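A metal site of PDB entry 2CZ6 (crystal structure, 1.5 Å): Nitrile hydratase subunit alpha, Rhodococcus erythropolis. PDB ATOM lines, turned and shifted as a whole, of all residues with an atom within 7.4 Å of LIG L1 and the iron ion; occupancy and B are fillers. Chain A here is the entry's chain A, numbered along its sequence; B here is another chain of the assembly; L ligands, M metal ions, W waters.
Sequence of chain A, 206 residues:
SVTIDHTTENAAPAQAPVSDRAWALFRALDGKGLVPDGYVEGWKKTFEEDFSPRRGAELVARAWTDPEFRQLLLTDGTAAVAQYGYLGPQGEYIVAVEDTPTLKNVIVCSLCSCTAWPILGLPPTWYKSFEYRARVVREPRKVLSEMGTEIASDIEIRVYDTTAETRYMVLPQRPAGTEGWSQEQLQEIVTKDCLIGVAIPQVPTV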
ATOM      1  N   GLN A  90     -30.836 -11.736 -35.214  1.00  0.00           N
ATOM      2  CA  GLN A  90     -30.961 -12.311 -33.871  1.00  0.00           C
ATOM      3  C   GLN A  90     -32.367 -12.146 -33.311  1.00  0.00           C
ATOM      4  O   GLN A  90     -32.581 -12.041 -32.107  1.00  0.00           O
ATOM      5  CB  GLN A  90     -29.894 -11.752 -32.923  1.00  0.00           C
ATOM      6  CG  GLN A  90     -28.488 -12.133 -33.364  1.00  0.00           C
ATOM      7  CD  GLN A  90     -28.305 -13.627 -33.365  1.00  0.00           C
ATOM      8  OE1 GLN A  90     -28.520 -14.273 -32.354  1.00  0.00           O
ATOM      9  NE2 GLN A  90     -27.921 -14.184 -34.507  1.00  0.00           N
ATOM     10  N   VAL A 108     -31.733 -16.633 -20.543  1.00  0.00           N
ATOM     11  CA  VAL A 108     -30.273 -16.534 -20.516  1.00  0.00           C
ATOM     12  C   VAL A 108     -29.726 -17.158 -21.802  1.00  0.00           C
ATOM     13  O   VAL A 108     -30.437 -17.903 -22.495  1.00  0.00           O
ATOM     14  CB  VAL A 108     -29.678 -17.266 -19.274  1.00  0.00           C
ATOM     15  CG1 VAL A 108     -29.982 -18.759 -19.315  1.00  0.00           C
ATOM     16  CG2 VAL A 108     -28.170 -17.031 -19.154  1.00  0.00           C
ATOM     17  N   CYS A 109     -28.470 -16.859 -22.098  1.00  0.00           N
ATOM     18  CA  CYS A 109     -27.669 -17.672 -22.997  1.00  0.00           C
ATOM     19  C   CYS A 109     -26.436 -18.127 -22.231  1.00  0.00           C
ATOM     20  O   CYS A 109     -25.452 -17.392 -22.101  1.00  0.00           O
ATOM     21  CB  CYS A 109     -27.264 -16.886 -24.227  1.00  0.00           C
ATOM     22  SG  CYS A 109     -26.227 -17.815 -25.385  1.00  0.00           S
ATOM     23  N   SER A 110     -26.490 -19.351 -21.694  1.00  0.00           N
ATOM     24  CA  SER A 110     -25.418 -19.801 -20.853  1.00  0.00           C
ATOM     25  C   SER A 110     -24.127 -19.972 -21.638  1.00  0.00           C
ATOM     26  O   SER A 110     -23.022 -19.839 -21.096  1.00  0.00           O
ATOM     27  CB  SER A 110     -25.775 -21.093 -20.113  1.00  0.00           C
ATOM     28  OG  SER A 110     -25.829 -22.195 -20.989  1.00  0.00           O
ATOM     29  N   LEU A 111     -24.272 -20.245 -22.935  1.00  0.00           N
ATOM     30  CA  LEU A 111     -23.111 -20.505 -23.780  1.00  0.00           C
ATOM     31  C   LEU A 111     -22.429 -19.272 -24.366  1.00  0.00           C
ATOM     32  O   LEU A 111     -21.296 -19.387 -24.853  1.00  0.00           O
ATOM     33  CB  LEU A 111     -23.484 -21.500 -24.876  1.00  0.00           C
ATOM     34  CG  LEU A 111     -23.934 -22.889 -24.398  1.00  0.00           C
ATOM     35  CD1 LEU A 111     -24.630 -23.654 -25.535  1.00  0.00           C
ATOM     36  CD2 LEU A 111     -22.750 -23.686 -23.837  1.00  0.00           C
ATOM     37  N   CSD A 112     -23.093 -18.109 -24.314  1.00  0.00           N
ATOM     38  CA  CSD A 112     -22.386 -16.821 -24.872  1.00  0.00           C
ATOM     39  CB  CSD A 112     -22.172 -17.068 -26.322  1.00  0.00           C
ATOM     40  SG  CSD A 112     -23.701 -17.643 -27.373  1.00  0.00           S
ATOM     41  C   CSD A 112     -23.391 -15.625 -24.573  1.00  0.00           C
ATOM     42  O   CSD A 112     -23.124 -14.985 -23.553  1.00  0.00           O
ATOM     43  OD1 CSD A 112     -23.251 -17.569 -28.727  1.00  0.00           O
ATOM     44  OD2 CSD A 112     -23.904 -19.075 -26.950  1.00  0.00           O
ATOM     45  N   SER A 113     -24.395 -15.264 -25.379  1.00  0.00           N
ATOM     46  CA  SER A 113     -25.113 -14.005 -25.099  1.00  0.00           C
ATOM     47  C   SER A 113     -26.457 -13.919 -25.803  1.00  0.00           C
ATOM     48  O   SER A 113     -27.149 -12.885 -25.720  1.00  0.00           O
ATOM     49  CB  SER A 113     -24.258 -12.783 -25.478  1.00  0.00           C
ATOM     50  OG  SER A 113     -24.108 -12.698 -26.877  1.00  0.00           O
ATOM     51  N   CSO A 114     -26.829 -15.003 -26.474  1.00  0.00           N
ATOM     52  CA  CSO A 114     -28.007 -15.046 -27.337  1.00  0.00           C
ATOM     53  CB  CSO A 114     -28.278 -16.488 -27.778  1.00  0.00           C
ATOM     54  SG  CSO A 114     -26.789 -17.274 -28.344  1.00  0.00           S
ATOM     55  C   CSO A 114     -29.209 -14.362 -26.722  1.00  0.00           C
ATOM     56  O   CSO A 114     -29.608 -14.665 -25.593  1.00  0.00           O
ATOM     57  OD  CSO A 114     -26.584 -16.707 -29.731  1.00  0.00           O
ATOM     58  N   THR A 115     -29.760 -13.429 -27.505  1.00  0.00           N
ATOM     59  CA  THR A 115     -30.776 -12.452 -27.073  1.00  0.00           C
ATOM     60  C   THR A 115     -31.557 -12.019 -28.303  1.00  0.00           C
ATOM     61  O   THR A 115     -30.984 -11.897 -29.391  1.00  0.00           O
ATOM     62  CB  THR A 115     -30.070 -11.201 -26.516  1.00  0.00           C
ATOM     63  OG1 THR A 115     -29.439 -11.524 -25.274  1.00  0.00           O
ATOM     64  CG2 THR A 115     -31.042 -10.027 -26.284  1.00  0.00           C
ATOM     65  N   TRP A 117     -32.284  -9.464 -30.064  1.00  0.00           N
ATOM     66  CA  TRP A 117     -31.807  -8.094 -30.235  1.00  0.00           C
ATOM     67  C   TRP A 117     -32.827  -7.036 -30.674  1.00  0.00           C
ATOM     68  O   TRP A 117     -32.871  -5.964 -30.097  1.00  0.00           O
ATOM     69  CB  TRP A 117     -30.676  -8.039 -31.255  1.00  0.00           C
ATOM     70  CG  TRP A 117     -29.378  -8.667 -30.865  1.00  0.00           C
ATOM     71  CD1 TRP A 117     -29.010  -9.180 -29.639  1.00  0.00           C
ATOM     72  CD2 TRP A 117     -28.252  -8.825 -31.720  1.00  0.00           C
ATOM     73  NE1 TRP A 117     -27.716  -9.652 -29.700  1.00  0.00           N
ATOM     74  CE2 TRP A 117     -27.234  -9.457 -30.970  1.00  0.00           C
ATOM     75  CE3 TRP A 117     -27.999  -8.507 -33.060  1.00  0.00           C
ATOM     76  CZ2 TRP A 117     -25.975  -9.762 -31.513  1.00  0.00           C
ATOM     77  CZ3 TRP A 117     -26.756  -8.813 -33.609  1.00  0.00           C
ATOM     78  CH2 TRP A 117     -25.763  -9.427 -32.827  1.00  0.00           C
ATOM     79  N   PRO A 123     -27.772  -7.343 -25.632  1.00  0.00           N
ATOM     80  CA  PRO A 123     -27.748  -7.720 -24.220  1.00  0.00           C
ATOM     81  C   PRO A 123     -26.879  -6.760 -23.403  1.00  0.00           C
ATOM     82  O   PRO A 123     -25.883  -6.249 -23.899  1.00  0.00           O
ATOM     83  CB  PRO A 123     -27.134  -9.122 -24.230  1.00  0.00           C
ATOM     84  CG  PRO A 123     -26.375  -9.180 -25.526  1.00  0.00           C
ATOM     85  CD  PRO A 123     -27.223  -8.407 -26.480  1.00  0.00           C
ATOM     86  N   TYR A 127     -25.820  -9.483 -18.387  1.00  0.00           N
ATOM     87  CA  TYR A 127     -26.459 -10.660 -18.944  1.00  0.00           C
ATOM     88  C   TYR A 127     -25.407 -11.556 -19.579  1.00  0.00           C
ATOM     89  O   TYR A 127     -25.557 -12.776 -19.630  1.00  0.00           O
ATOM     90  CB  TYR A 127     -27.499 -10.215 -19.975  1.00  0.00           C
ATOM     91  CG  TYR A 127     -28.226 -11.281 -20.738  1.00  0.00           C
ATOM     92  CD1 TYR A 127     -27.706 -11.802 -21.929  1.00  0.00           C
ATOM     93  CD2 TYR A 127     -29.469 -11.743 -20.323  1.00  0.00           C
ATOM     94  CE1 TYR A 127     -28.392 -12.750 -22.676  1.00  0.00           C
ATOM     95  CE2 TYR A 127     -30.173 -12.716 -21.039  1.00  0.00           C
ATOM     96  CZ  TYR A 127     -29.627 -13.207 -22.220  1.00  0.00           C
ATOM     97  OH  TYR A 127     -30.339 -14.148 -22.948  1.00  0.00           O
ATOM     98  N   LYS A 128     -24.338 -10.924 -20.078  1.00  0.00           N
ATOM     99  CA  LYS A 128     -23.216 -11.625 -20.696  1.00  0.00           C
ATOM    100  C   LYS A 128     -22.166 -12.052 -19.674  1.00  0.00           C
ATOM    101  O   LYS A 128     -21.188 -12.703 -20.042  1.00  0.00           O
ATOM    102  CB  LYS A 128     -22.579 -10.717 -21.748  1.00  0.00           C
ATOM    103  CG  LYS A 128     -23.511 -10.446 -22.933  1.00  0.00           C
ATOM    104  CD  LYS A 128     -22.958  -9.404 -23.889  1.00  0.00           C
ATOM    105  CE  LYS A 128     -23.047  -7.986 -23.358  1.00  0.00           C
ATOM    106  NZ  LYS A 128     -22.674  -6.958 -24.375  1.00  0.00           N
ATOM    107  N   ARG A 133     -24.432 -16.194 -16.530  1.00  0.00           N
ATOM    108  CA  ARG A 133     -24.362 -17.400 -17.367  1.00  0.00           C
ATOM    109  C   ARG A 133     -24.178 -18.697 -16.581  1.00  0.00           C
ATOM    110  O   ARG A 133     -24.755 -19.726 -16.941  1.00  0.00           O
ATOM    111  CB  ARG A 133     -23.250 -17.243 -18.422  1.00  0.00           C
ATOM    112  CG  ARG A 133     -23.597 -16.191 -19.475  1.00  0.00           C
ATOM    113  CD  ARG A 133     -22.451 -15.938 -20.432  1.00  0.00           C
ATOM    114  NE  ARG A 133     -21.942 -17.208 -20.934  1.00  0.00           N
ATOM    115  CZ  ARG A 133     -20.724 -17.410 -21.443  1.00  0.00           C
ATOM    116  NH1 ARG A 133     -19.882 -16.398 -21.592  1.00  0.00           N
ATOM    117  NH2 ARG A 133     -20.372 -18.630 -21.818  1.00  0.00           N
ATOM    118  N   THR A 162     -31.033 -19.971 -24.149  1.00  0.00           N
ATOM    119  CA  THR A 162     -31.119 -19.672 -25.573  1.00  0.00           C
ATOM    120  C   THR A 162     -29.967 -20.328 -26.317  1.00  0.00           C
ATOM    121  O   THR A 162     -28.927 -19.721 -26.570  1.00  0.00           O
ATOM    122  CB  THR A 162     -31.133 -18.135 -25.798  1.00  0.00           C
ATOM    123  OG1 THR A 162     -32.136 -17.544 -24.961  1.00  0.00           O
ATOM    124  CG2 THR A 162     -31.419 -17.787 -27.253  1.00  0.00           C
ATOM    125  N   THR A 163     -30.173 -21.596 -26.661  1.00  0.00           N
ATOM    126  CA  THR A 163     -29.101 -22.436 -27.193  1.00  0.00           C
ATOM    127  C   THR A 163     -29.147 -22.650 -28.693  1.00  0.00           C
ATOM    128  O   THR A 163     -28.225 -23.229 -29.252  1.00  0.00           O
ATOM    129  CB  THR A 163     -29.105 -23.814 -26.492  1.00  0.00           C
ATOM    130  OG1 THR A 163     -30.453 -24.321 -26.484  1.00  0.00           O
ATOM    131  CG2 THR A 163     -28.623 -23.685 -25.053  1.00  0.00           C
ATOM    132  N   ARG A 167     -35.530 -17.038 -30.313  1.00  0.00           N
ATOM    133  CA  ARG A 167     -35.175 -15.818 -29.607  1.00  0.00           C
ATOM    134  C   ARG A 167     -36.384 -15.422 -28.770  1.00  0.00           C
ATOM    135  O   ARG A 167     -37.499 -15.275 -29.288  1.00  0.00           O
ATOM    136  CB  ARG A 167     -34.747 -14.732 -30.593  1.00  0.00           C
ATOM    137  CG  ARG A 167     -33.427 -15.052 -31.304  1.00  0.00           C
ATOM    138  CD  ARG A 167     -32.215 -14.874 -30.377  1.00  0.00           C
ATOM    139  NE  ARG A 167     -30.984 -15.317 -31.029  1.00  0.00           N
ATOM    140  CZ  ARG A 167     -30.579 -16.574 -31.098  1.00  0.00           C
ATOM    141  NH1 ARG A 167     -31.284 -17.540 -30.529  1.00  0.00           N
ATOM    142  NH2 ARG A 167     -29.462 -16.871 -31.739  1.00  0.00           N
ATOM    143  N   TYR B  37     -19.254  -6.996 -33.890  1.00  0.00           N
ATOM    144  CA  TYR B  37     -20.523  -7.418 -34.477  1.00  0.00           C
ATOM    145  C   TYR B  37     -20.627  -6.968 -35.926  1.00  0.00           C
ATOM    146  O   TYR B  37     -21.057  -7.728 -36.792  1.00  0.00           O
ATOM    147  CB  TYR B  37     -21.723  -6.864 -33.702  1.00  0.00           C
ATOM    148  CG  TYR B  37     -22.091  -7.570 -32.400  1.00  0.00           C
ATOM    149  CD1 TYR B  37     -21.400  -8.684 -31.929  1.00  0.00           C
ATOM    150  CD2 TYR B  37     -23.161  -7.099 -31.667  1.00  0.00           C
ATOM    151  CE1 TYR B  37     -21.789  -9.320 -30.732  1.00  0.00           C
ATOM    152  CE2 TYR B  37     -23.553  -7.707 -30.495  1.00  0.00           C
ATOM    153  CZ  TYR B  37     -22.866  -8.805 -30.030  1.00  0.00           C
ATOM    154  OH  TYR B  37     -23.319  -9.368 -28.862  1.00  0.00           O
ATOM    155  N   VAL B  52     -22.332 -17.661 -38.904  1.00  0.00           N
ATOM    156  CA  VAL B  52     -22.487 -17.193 -37.536  1.00  0.00           C
ATOM    157  C   VAL B  52     -22.025 -18.291 -36.566  1.00  0.00           C
ATOM    158  O   VAL B  52     -21.362 -18.006 -35.574  1.00  0.00           O
ATOM    159  CB  VAL B  52     -23.926 -16.720 -37.267  1.00  0.00           C
ATOM    160  CG1 VAL B  52     -24.145 -16.433 -35.775  1.00  0.00           C
ATOM    161  CG2 VAL B  52     -24.242 -15.473 -38.094  1.00  0.00           C
ATOM    162  N   ARG B  56     -19.343 -18.415 -33.162  1.00  0.00           N
ATOM    163  CA  ARG B  56     -19.499 -18.979 -31.820  1.00  0.00           C
ATOM    164  C   ARG B  56     -18.357 -19.949 -31.520  1.00  0.00           C
ATOM    165  O   ARG B  56     -17.743 -19.892 -30.440  1.00  0.00           O
ATOM    166  CB  ARG B  56     -20.832 -19.714 -31.667  1.00  0.00           C
ATOM    167  CG  ARG B  56     -22.038 -18.816 -31.754  1.00  0.00           C
ATOM    168  CD  ARG B  56     -23.284 -19.529 -31.227  1.00  0.00           C
ATOM    169  NE  ARG B  56     -24.417 -18.623 -31.310  1.00  0.00           N
ATOM    170  CZ  ARG B  56     -25.191 -18.486 -32.388  1.00  0.00           C
ATOM    171  NH1 ARG B  56     -24.959 -19.233 -33.470  1.00  0.00           N
ATOM    172  NH2 ARG B  56     -26.175 -17.594 -32.376  1.00  0.00           N
ATOM    173  N   TYR B  72     -16.254  -9.476 -22.994  1.00  0.00           N
ATOM    174  CA  TYR B  72     -17.130  -9.987 -24.035  1.00  0.00           C
ATOM    175  C   TYR B  72     -16.794  -9.466 -25.435  1.00  0.00           C
ATOM    176  O   TYR B  72     -16.487 -10.249 -26.344  1.00  0.00           O
ATOM    177  CB  TYR B  72     -18.591  -9.673 -23.701  1.00  0.00           C
ATOM    178  CG  TYR B  72     -19.546 -10.125 -24.782  1.00  0.00           C
ATOM    179  CD1 TYR B  72     -20.088 -11.404 -24.763  1.00  0.00           C
ATOM    180  CD2 TYR B  72     -19.849  -9.290 -25.855  1.00  0.00           C
ATOM    181  CE1 TYR B  72     -20.944 -11.832 -25.747  1.00  0.00           C
ATOM    182  CE2 TYR B  72     -20.699  -9.709 -26.870  1.00  0.00           C
ATOM    183  CZ  TYR B  72     -21.258 -10.979 -26.814  1.00  0.00           C
ATOM    184  OH  TYR B  72     -22.093 -11.421 -27.817  1.00  0.00           O
ATOM    185  N   TYR B  76     -14.918 -11.252 -29.293  1.00  0.00           N
ATOM    186  CA  TYR B  76     -15.397 -11.261 -30.684  1.00  0.00           C
ATOM    187  C   TYR B  76     -14.461 -10.553 -31.649  1.00  0.00           C
ATOM    188  O   TYR B  76     -14.354 -10.968 -32.791  1.00  0.00           O
ATOM    189  CB  TYR B  76     -16.864 -10.816 -30.795  1.00  0.00           C
ATOM    190  CG  TYR B  76     -17.740 -11.810 -30.060  1.00  0.00           C
ATOM    191  CD1 TYR B  76     -18.278 -12.922 -30.704  1.00  0.00           C
ATOM    192  CD2 TYR B  76     -17.924 -11.696 -28.681  1.00  0.00           C
ATOM    193  CE1 TYR B  76     -19.036 -13.878 -30.002  1.00  0.00           C
ATOM    194  CE2 TYR B  76     -18.662 -12.641 -27.982  1.00  0.00           C
ATOM    195  CZ  TYR B  76     -19.222 -13.724 -28.635  1.00  0.00           C
ATOM    196  OH  TYR B  76     -19.942 -14.646 -27.903  1.00  0.00           O
ATOM    197  N   ARG B 141     -24.310 -27.209 -29.864  1.00  0.00           N
ATOM    198  CA  ARG B 141     -25.223 -26.319 -29.141  1.00  0.00           C
ATOM    199  C   ARG B 141     -26.000 -27.062 -28.056  1.00  0.00           C
ATOM    200  O   ARG B 141     -27.215 -26.925 -27.914  1.00  0.00           O
ATOM    201  CB  ARG B 141     -26.142 -25.580 -30.114  1.00  0.00           C
ATOM    202  CG  ARG B 141     -25.392 -24.587 -30.986  1.00  0.00           C
ATOM    203  CD  ARG B 141     -24.584 -23.621 -30.140  1.00  0.00           C
ATOM    204  NE  ARG B 141     -25.455 -22.674 -29.446  1.00  0.00           N
ATOM    205  CZ  ARG B 141     -25.006 -21.701 -28.652  1.00  0.00           C
ATOM    206  NH1 ARG B 141     -23.702 -21.606 -28.404  1.00  0.00           N
ATOM    207  NH2 ARG B 141     -25.863 -20.859 -28.113  1.00  0.00           N
HETATM  208  N1  LIG L   1     -24.767 -15.242 -28.179  1.00  0.00           N
HETATM  209  O1  LIG L   1     -24.186 -14.720 -29.104  1.00  0.00           O
HETATM  210  C1  LG2 L   2     -24.617 -14.368 -32.682  1.00  0.00           C
HETATM  211  C2  LG2 L   2     -23.413 -15.189 -32.216  1.00  0.00           C
HETATM  212  C3  LG2 L   2     -22.091 -14.423 -32.327  1.00  0.00           C
HETATM  213  C4  LG2 L   2     -22.134 -13.004 -31.723  1.00  0.00           C
HETATM  214  C5  LG2 L   2     -23.386 -12.222 -32.175  1.00  0.00           C
HETATM  215  C6  LG2 L   2     -24.680 -13.011 -31.992  1.00  0.00           C
HETATM  216  N1  LG2 L   2     -21.060 -12.235 -32.711  1.00  0.00           N
HETATM  217  C7  LG2 L   2     -20.260 -11.612 -33.363  1.00  0.00           C
HETATM  218 FE    FE M   1     -25.351 -16.258 -26.944  1.00  0.00          FE
HETATM  219  O   HOH W   1     -26.960 -13.760 -30.191  1.00  0.00           O
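OG of Ser 113 sits at hydrogen-bond distance from O1 of LIG L1 (3.0 Å).
The side-chain hydroxyl (OG) of Ser 113 lies within hydrogen-bond range of the side-chain hydroxyl (OH) of Tyr 72 of chain B, 2.6 Å away. OD of CSO 114 sits at hydrogen-bond distance from NH2 of Arg 56 of chain B (2.8 Å). OH of Tyr 127 sits at hydrogen-bond distance from N of Cys 109 (3.4 Å). The guanidinium group (NH2) of Arg 141 of chain B lies within salt-bridge range of OD2 of CSD 112 (2.9 Å). OD1 of CSD 112 is in salt-bridge range of NE of Arg 56 of chain B (3.0 Å). SG of CSO 114 sits close to the guanidinium group of Arg 141 of chain B (3.7 Å). The side-chain sulfur of Cys 109 lies close to the backbone carbonyl oxygen of Thr 162 (3.5 Å). The side-chain hydroxyl (OG1) of Thr 115 is in hydrogen-bond range of the backbone carbonyl oxygen (O) of Ser 113 (2.7 Å).
Four residues have an atom within 4 Å of the iron ion: Cys 109, CSD 112, Ser 113 and CSO 114.
The iron ion is bound by N1 of LIG L1 (1.7 Å). The iron ion is bound by N of CSO 114 (2.0 Å). N of Ser 113 binds the iron ion. SG of CSD 112 binds the iron ion (2.2 Å). SG of CSO 114 binds the iron ion (2.2 Å). The iron ion is bound by the side-chain sulfur (SG) of Cys 109, 2.4 Å away.
Water W1 lies within hydrogen-bond range of the side-chain amide oxygen of Gln 90, OD of CSO 114 and an oxygen (O1) of LIG L1.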
